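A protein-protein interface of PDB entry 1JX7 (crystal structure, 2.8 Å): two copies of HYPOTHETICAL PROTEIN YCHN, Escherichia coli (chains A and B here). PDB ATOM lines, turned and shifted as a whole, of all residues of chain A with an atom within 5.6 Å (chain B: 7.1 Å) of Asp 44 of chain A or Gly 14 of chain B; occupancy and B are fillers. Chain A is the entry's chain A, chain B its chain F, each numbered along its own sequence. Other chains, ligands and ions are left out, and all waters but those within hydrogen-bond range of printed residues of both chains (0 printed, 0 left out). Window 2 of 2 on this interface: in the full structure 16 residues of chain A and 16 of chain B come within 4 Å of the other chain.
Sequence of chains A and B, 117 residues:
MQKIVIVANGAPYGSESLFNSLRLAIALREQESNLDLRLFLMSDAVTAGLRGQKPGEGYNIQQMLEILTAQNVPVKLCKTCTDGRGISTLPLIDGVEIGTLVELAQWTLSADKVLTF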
ATOM      1  N   ASN A   9       6.449 -16.749  -1.210  1.00  0.00           N
ATOM      2  CA  ASN A   9       5.634 -15.621  -1.667  1.00  0.00           C
ATOM      3  C   ASN A   9       4.311 -16.102  -2.255  1.00  0.00           C
ATOM      4  O   ASN A   9       3.327 -15.364  -2.284  1.00  0.00           O
ATOM      5  CB  ASN A   9       6.394 -14.833  -2.740  1.00  0.00           C
ATOM      6  CG  ASN A   9       7.610 -14.107  -2.196  1.00  0.00           C
ATOM      7  OD1 ASN A   9       8.351 -14.639  -1.366  1.00  0.00           O
ATOM      8  ND2 ASN A   9       7.840 -12.889  -2.673  1.00  0.00           N
ATOM      9  N   GLY A  10       4.288 -17.350  -2.714  1.00  0.00           N
ATOM     10  CA  GLY A  10       3.103 -17.894  -3.349  1.00  0.00           C
ATOM     11  C   GLY A  10       1.800 -18.097  -2.580  1.00  0.00           C
ATOM     12  O   GLY A  10       1.796 -18.527  -1.426  1.00  0.00           O
ATOM     13  N   ALA A  11       0.692 -17.798  -3.245  1.00  0.00           N
ATOM     14  CA  ALA A  11      -0.633 -17.978  -2.654  1.00  0.00           C
ATOM     15  C   ALA A  11      -0.922 -19.471  -2.617  1.00  0.00           C
ATOM     16  O   ALA A  11      -0.629 -20.188  -3.580  1.00  0.00           O
ATOM     17  CB  ALA A  11      -1.699 -17.261  -3.489  1.00  0.00           C
ATOM     18  N   PRO A  12      -1.491 -19.958  -1.510  1.00  0.00           N
ATOM     19  CA  PRO A  12      -1.802 -21.387  -1.391  1.00  0.00           C
ATOM     20  C   PRO A  12      -2.699 -21.860  -2.526  1.00  0.00           C
ATOM     21  O   PRO A  12      -3.550 -21.109  -2.998  1.00  0.00           O
ATOM     22  CB  PRO A  12      -2.527 -21.475  -0.043  1.00  0.00           C
ATOM     23  CG  PRO A  12      -1.985 -20.319   0.717  1.00  0.00           C
ATOM     24  CD  PRO A  12      -1.888 -19.224  -0.296  1.00  0.00           C
ATOM     25  N   MET A  42       5.789 -14.530   3.143  1.00  0.00           N
ATOM     26  CA  MET A  42       5.519 -13.136   2.798  1.00  0.00           C
ATOM     27  C   MET A  42       4.311 -13.019   1.877  1.00  0.00           C
ATOM     28  O   MET A  42       3.734 -14.013   1.456  1.00  0.00           O
ATOM     29  CB  MET A  42       6.737 -12.502   2.108  1.00  0.00           C
ATOM     30  CG  MET A  42       7.980 -12.397   2.978  1.00  0.00           C
ATOM     31  SD  MET A  42       9.279 -11.428   2.227  1.00  0.00           S
ATOM     32  CE  MET A  42       9.636 -12.410   0.780  1.00  0.00           C
ATOM     33  N   SER A  43       3.945 -11.773   1.576  1.00  0.00           N
ATOM     34  CA  SER A  43       2.862 -11.472   0.693  1.00  0.00           C
ATOM     35  C   SER A  43       1.719 -12.481   0.691  1.00  0.00           C
ATOM     36  O   SER A  43       1.209 -12.827   1.759  1.00  0.00           O
ATOM     37  CB  SER A  43       3.369 -11.290  -0.724  1.00  0.00           C
ATOM     38  OG  SER A  43       3.890 -12.504  -1.228  1.00  0.00           O
ATOM     39  N   ASP A  44       1.305 -12.974  -0.473  1.00  0.00           N
ATOM     40  CA  ASP A  44       0.335 -14.042  -0.683  1.00  0.00           C
ATOM     41  C   ASP A  44       0.369 -15.363   0.092  1.00  0.00           C
ATOM     42  O   ASP A  44      -0.698 -15.882   0.470  1.00  0.00           O
ATOM     43  CB  ASP A  44       0.226 -14.380  -2.147  1.00  0.00           C
ATOM     44  CG  ASP A  44      -0.049 -13.170  -2.997  1.00  0.00           C
ATOM     45  OD1 ASP A  44      -0.211 -13.345  -4.219  1.00  0.00           O
ATOM     46  OD2 ASP A  44      -0.104 -12.046  -2.440  1.00  0.00           O
ATOM     47  N   ALA A  45       1.552 -15.910   0.346  1.00  0.00           N
ATOM     48  CA  ALA A  45       1.676 -17.181   1.068  1.00  0.00           C
ATOM     49  C   ALA A  45       1.163 -17.073   2.498  1.00  0.00           C
ATOM     50  O   ALA A  45       1.110 -18.054   3.226  1.00  0.00           O
ATOM     51  CB  ALA A  45       3.163 -17.650   1.079  1.00  0.00           C
ATOM     52  N   VAL A  46       0.763 -15.870   2.884  1.00  0.00           N
ATOM     53  CA  VAL A  46       0.304 -15.603   4.230  1.00  0.00           C
ATOM     54  C   VAL A  46      -1.090 -16.105   4.570  1.00  0.00           C
ATOM     55  O   VAL A  46      -1.390 -16.381   5.732  1.00  0.00           O
ATOM     56  CB  VAL A  46       0.413 -14.081   4.514  1.00  0.00           C
ATOM     57  CG1 VAL A  46      -0.518 -13.677   5.623  1.00  0.00           C
ATOM     58  CG2 VAL A  46       1.850 -13.748   4.892  1.00  0.00           C
ATOM     59  N   THR A  47      -1.957 -16.221   3.556  1.00  0.00           N
ATOM     60  CA  THR A  47      -3.310 -16.707   3.798  1.00  0.00           C
ATOM     61  C   THR A  47      -3.253 -18.200   4.099  1.00  0.00           C
ATOM     62  O   THR A  47      -4.207 -18.763   4.648  1.00  0.00           O
ATOM     63  CB  THR A  47      -4.247 -16.432   2.569  1.00  0.00           C
ATOM     64  OG1 THR A  47      -3.764 -17.123   1.412  1.00  0.00           O
ATOM     65  CG2 THR A  47      -4.301 -14.958   2.252  1.00  0.00           C
ATOM     66  N   ALA A  48      -2.121 -18.820   3.765  1.00  0.00           N
ATOM     67  CA  ALA A  48      -1.891 -20.246   4.014  1.00  0.00           C
ATOM     68  C   ALA A  48      -1.964 -20.594   5.508  1.00  0.00           C
ATOM     69  O   ALA A  48      -2.064 -21.765   5.896  1.00  0.00           O
ATOM     70  CB  ALA A  48      -0.539 -20.635   3.470  1.00  0.00           C
ATOM     71  N   CYS A  81       1.925  -7.960   5.764  1.00  0.00           N
ATOM     72  CA  CYS A  81       1.149  -8.725   4.799  1.00  0.00           C
ATOM     73  C   CYS A  81      -0.191  -9.182   5.369  1.00  0.00           C
ATOM     74  O   CYS A  81      -1.234  -8.956   4.759  1.00  0.00           O
ATOM     75  CB  CYS A  81       1.953  -9.943   4.317  1.00  0.00           C
ATOM     76  SG  CYS A  81       3.439  -9.538   3.363  1.00  0.00           S
ATOM     77  N   ARG A  85      -4.379  -8.180   4.494  1.00  0.00           N
ATOM     78  CA  ARG A  85      -5.371  -9.153   4.058  1.00  0.00           C
ATOM     79  C   ARG A  85      -6.403  -9.489   5.152  1.00  0.00           C
ATOM     80  O   ARG A  85      -7.254 -10.359   4.967  1.00  0.00           O
ATOM     81  CB  ARG A  85      -4.660 -10.412   3.550  1.00  0.00           C
ATOM     82  CG  ARG A  85      -3.243 -10.131   3.069  1.00  0.00           C
ATOM     83  CD  ARG A  85      -2.863 -10.745   1.732  1.00  0.00           C
ATOM     84  NE  ARG A  85      -1.564 -10.218   1.298  1.00  0.00           N
ATOM     85  CZ  ARG A  85      -1.058 -10.342   0.067  1.00  0.00           C
ATOM     86  NH1 ARG A  85      -1.737 -10.978  -0.880  1.00  0.00           N
ATOM     87  NH2 ARG A  85       0.121  -9.812  -0.221  1.00  0.00           N
ATOM     88  N   GLY B  10      -6.608 -13.431  -9.754  1.00  0.00           N
ATOM     89  CA  GLY B  10      -5.418 -13.159  -8.969  1.00  0.00           C
ATOM     90  C   GLY B  10      -5.609 -12.856  -7.488  1.00  0.00           C
ATOM     91  O   GLY B  10      -6.675 -12.429  -7.067  1.00  0.00           O
ATOM     92  N   ALA B  11      -4.551 -13.069  -6.714  1.00  0.00           N
ATOM     93  CA  ALA B  11      -4.588 -12.830  -5.276  1.00  0.00           C
ATOM     94  C   ALA B  11      -4.549 -11.344  -4.949  1.00  0.00           C
ATOM     95  O   ALA B  11      -3.872 -10.568  -5.611  1.00  0.00           O
ATOM     96  CB  ALA B  11      -3.414 -13.544  -4.590  1.00  0.00           C
ATOM     97  N   PRO B  12      -5.275 -10.929  -3.909  1.00  0.00           N
ATOM     98  CA  PRO B  12      -5.308  -9.517  -3.515  1.00  0.00           C
ATOM     99  C   PRO B  12      -3.939  -8.985  -3.068  1.00  0.00           C
ATOM    100  O   PRO B  12      -3.221  -9.645  -2.324  1.00  0.00           O
ATOM    101  CB  PRO B  12      -6.329  -9.502  -2.382  1.00  0.00           C
ATOM    102  CG  PRO B  12      -7.240 -10.628  -2.729  1.00  0.00           C
ATOM    103  CD  PRO B  12      -6.270 -11.705  -3.145  1.00  0.00           C
ATOM    104  N   TYR B  13      -3.591  -7.789  -3.528  1.00  0.00           N
ATOM    105  CA  TYR B  13      -2.330  -7.139  -3.179  1.00  0.00           C
ATOM    106  C   TYR B  13      -1.098  -7.823  -3.779  1.00  0.00           C
ATOM    107  O   TYR B  13      -0.048  -7.215  -3.912  1.00  0.00           O
ATOM    108  CB  TYR B  13      -2.190  -7.052  -1.662  1.00  0.00           C
ATOM    109  CG  TYR B  13      -3.383  -6.433  -0.974  1.00  0.00           C
ATOM    110  CD1 TYR B  13      -3.666  -5.074  -1.110  1.00  0.00           C
ATOM    111  CD2 TYR B  13      -4.258  -7.216  -0.204  1.00  0.00           C
ATOM    112  CE1 TYR B  13      -4.787  -4.505  -0.497  1.00  0.00           C
ATOM    113  CE2 TYR B  13      -5.379  -6.660   0.412  1.00  0.00           C
ATOM    114  CZ  TYR B  13      -5.642  -5.305   0.255  1.00  0.00           C
ATOM    115  OH  TYR B  13      -6.768  -4.753   0.833  1.00  0.00           O
ATOM    116  N   GLY B  14      -1.230  -9.098  -4.130  1.00  0.00           N
ATOM    117  CA  GLY B  14      -0.100  -9.800  -4.700  1.00  0.00           C
ATOM    118  C   GLY B  14       0.258  -9.250  -6.064  1.00  0.00           C
ATOM    119  O   GLY B  14       1.434  -9.162  -6.423  1.00  0.00           O
ATOM    120  N   SER B  15      -0.768  -8.871  -6.826  1.00  0.00           N
ATOM    121  CA  SER B  15      -0.573  -8.326  -8.161  1.00  0.00           C
ATOM    122  C   SER B  15      -1.681  -7.336  -8.519  1.00  0.00           C
ATOM    123  O   SER B  15      -2.782  -7.390  -7.958  1.00  0.00           O
ATOM    124  CB  SER B  15      -0.570  -9.453  -9.190  1.00  0.00           C
ATOM    125  OG  SER B  15      -1.873  -9.969  -9.375  1.00  0.00           O
ATOM    126  N   GLU B  16      -1.378  -6.448  -9.458  1.00  0.00           N
ATOM    127  CA  GLU B  16      -2.332  -5.447  -9.927  1.00  0.00           C
ATOM    128  C   GLU B  16      -3.484  -6.141 -10.639  1.00  0.00           C
ATOM    129  O   GLU B  16      -4.520  -5.535 -10.905  1.00  0.00           O
ATOM    130  CB  GLU B  16      -1.650  -4.469 -10.893  1.00  0.00           C
ATOM    131  CG  GLU B  16      -0.793  -3.398 -10.223  1.00  0.00           C
ATOM    132  CD  GLU B  16      -0.035  -2.539 -11.236  1.00  0.00           C
ATOM    133  OE1 GLU B  16       1.002  -3.007 -11.756  1.00  0.00           O
ATOM    134  OE2 GLU B  16      -0.476  -1.405 -11.520  1.00  0.00           O
ATOM    135  N   SER B  17      -3.298  -7.416 -10.934  1.00  0.00           N
ATOM    136  CA  SER B  17      -4.304  -8.199 -11.638  1.00  0.00           C
ATOM    137  C   SER B  17      -5.717  -8.023 -11.093  1.00  0.00           C
ATOM    138  O   SER B  17      -6.625  -7.653 -11.841  1.00  0.00           O
ATOM    139  CB  SER B  17      -3.916  -9.676 -11.615  1.00  0.00           C
ATOM    140  OG  SER B  17      -4.714 -10.407 -12.521  1.00  0.00           O
ATOM    141  N   ASP B  44      -7.293 -18.041  -5.988  1.00  0.00           N
ATOM    142  CA  ASP B  44      -6.618 -17.075  -5.126  1.00  0.00           C
ATOM    143  C   ASP B  44      -7.269 -15.719  -4.874  1.00  0.00           C
ATOM    144  O   ASP B  44      -6.950 -15.051  -3.885  1.00  0.00           O
ATOM    145  CB  ASP B  44      -5.180 -16.847  -5.599  1.00  0.00           C
ATOM    146  CG  ASP B  44      -4.405 -18.136  -5.745  1.00  0.00           C
ATOM    147  OD1 ASP B  44      -4.751 -19.120  -5.054  1.00  0.00           O
ATOM    148  OD2 ASP B  44      -3.444 -18.156  -6.545  1.00  0.00           O
ATOM    149  N   THR B  47      -9.886 -14.839  -1.449  1.00  0.00           N
ATOM    150  CA  THR B  47      -9.551 -14.256  -0.144  1.00  0.00           C
ATOM    151  C   THR B  47      -9.787 -12.736  -0.087  1.00  0.00           C
ATOM    152  O   THR B  47      -9.735 -12.128   0.985  1.00  0.00           O
ATOM    153  CB  THR B  47      -8.084 -14.573   0.225  1.00  0.00           C
ATOM    154  OG1 THR B  47      -7.225 -14.156  -0.846  1.00  0.00           O
ATOM    155  CG2 THR B  47      -7.899 -16.069   0.457  1.00  0.00           C
ATOM    156  N   TYR B  59      -3.627   1.045  -2.243  1.00  0.00           N
ATOM    157  CA  TYR B  59      -5.050   0.769  -2.335  1.00  0.00           C
ATOM    158  C   TYR B  59      -5.567  -0.262  -1.339  1.00  0.00           C
ATOM    159  O   TYR B  59      -4.817  -1.072  -0.810  1.00  0.00           O
ATOM    160  CB  TYR B  59      -5.404   0.331  -3.757  1.00  0.00           C
ATOM    161  CG  TYR B  59      -4.682  -0.908  -4.233  1.00  0.00           C
ATOM    162  CD1 TYR B  59      -5.137  -2.181  -3.900  1.00  0.00           C
ATOM    163  CD2 TYR B  59      -3.544  -0.806  -5.029  1.00  0.00           C
ATOM    164  CE1 TYR B  59      -4.483  -3.323  -4.359  1.00  0.00           C
ATOM    165  CE2 TYR B  59      -2.880  -1.938  -5.491  1.00  0.00           C
ATOM    166  CZ  TYR B  59      -3.348  -3.188  -5.151  1.00  0.00           C
ATOM    167  OH  TYR B  59      -2.693  -4.302  -5.626  1.00  0.00           O
ATOM    168  N   ILE B  61      -8.360  -3.154  -1.190  1.00  0.00           N
ATOM    169  CA  ILE B  61      -9.288  -3.996  -1.919  1.00  0.00           C
ATOM    170  C   ILE B  61     -10.670  -4.174  -1.294  1.00  0.00           C
ATOM    171  O   ILE B  61     -11.647  -4.354  -2.009  1.00  0.00           O
ATOM    172  CB  ILE B  61      -8.634  -5.361  -2.185  1.00  0.00           C
ATOM    173  CG1 ILE B  61      -7.938  -5.303  -3.528  1.00  0.00           C
ATOM    174  CG2 ILE B  61      -9.670  -6.481  -2.137  1.00  0.00           C
ATOM    175  CD1 ILE B  61      -7.010  -6.430  -3.744  1.00  0.00           C
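The backbone carbonyl oxygen (O) of Pro 12 of chain A sits close to the side-chain carboxylate (OD1) of Asp 44 of chain B. The guanidinium group of Arg 85 of chain A sits at hydrogen-bond distance from the backbone carbonyl oxygen of Pro 12 of chain B (2.5 Å).
The side-chain hydroxyl (OG1) of Thr 47 of chain A is in hydrogen-bond range of the backbone carbonyl oxygen (O) of Asp 44 of chain A, 3.4 Å away. The side-chain carboxylate (OD2) of Asp 44 of chain A is in salt-bridge range of the guanidinium group (NH1) of Arg 85 of chain A. The backbone NH of Ile 61 of chain B lies within hydrogen-bond range of the side-chain hydroxyl of Tyr 13 of chain B (3.0 Å). OG1 of Thr 47 of chain B is in hydrogen-bond range of O of Asp 44 of chain B.
Among the printed residues, pairs that only touch across the chains: Asp 44 of chain A with Gly 14 of chain B (3.2 Å), Asp 44 of chain A with Ala 11 of chain B (3.2 Å), Ala 11 of chain A with Asp 44 of chain B (3.6 Å), Arg 85 of chain A with Gly 14 of chain B (3.8 Å), Arg 85 of chain A with Tyr 13 of chain B (3.9 Å) and Asp 44 of chain A with Pro 12 of chain B (3.9 Å).
Asp 44 of chain A touches just these residues of chain B: Ala 11 (3.2 Å), Pro 12 (3.9 Å) and Gly 14 (3.2 Å). Gly 14 of chain B touches just these residues of chain A: Asp 44 (3.2 Å) and Arg 85 (3.8 Å). Of the printed residues of chain B, Pro 12 of chain A touches Asp 44 (3.1 Å). Of the printed residues of chain A, Tyr 13 of chain B touches Arg 85 (3.9 Å). Printed residues of chain B within 4 Å of Ala 11 of chain A: Asp 44 (3.6 Å). Of the printed residues of chain B, Arg 85 of chain A touches Pro 12 (2.5 Å), Tyr 13 (3.9 Å) and Gly 14 (3.8 Å). Val 46 of chain A touches none of the printed residues of chain B. Ala 48 of chain A touches none of the printed residues of chain B. The nearest residue of chain B that does not touch Asp 44 of chain A is Tyr 13 of chain B (4.5 Å). The nearest residue of chain A that does not touch Gly 14 of chain B is Ser 43 of chain A (5.5 Å). The nearest printed residue of chain A that does not touch Pro 12 of chain B is Ser 43 of chain A (6.4 Å).
Printed residues of chain A that touch a printed residue of chain B: Ala 11, Pro 12, Asp 44 and Arg 85. Hydrophobic or aromatic side chains of chain A that line the printed part of chain B: Ala 11. Of the 12 printed residues of chain B, 5 touch a printed residue of chain A. Among the printed residues, 8 pairs touch across the chains. Among the printed residues, no Asp or Glu carboxylate lies within 4 Å of a Lys or Arg side-chain nitrogen of the other chain.
Ala 11 of chain A touches Asp 44 of chain B, and with the chains exchanged Asp 44 of chain A touches Ala 11 of chain B. Pro 12 of chain A touches Asp 44 of chain B, and with the chains exchanged Asp 44 of chain A touches Pro 12 of chain B. 5 positions are printed for both chains.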
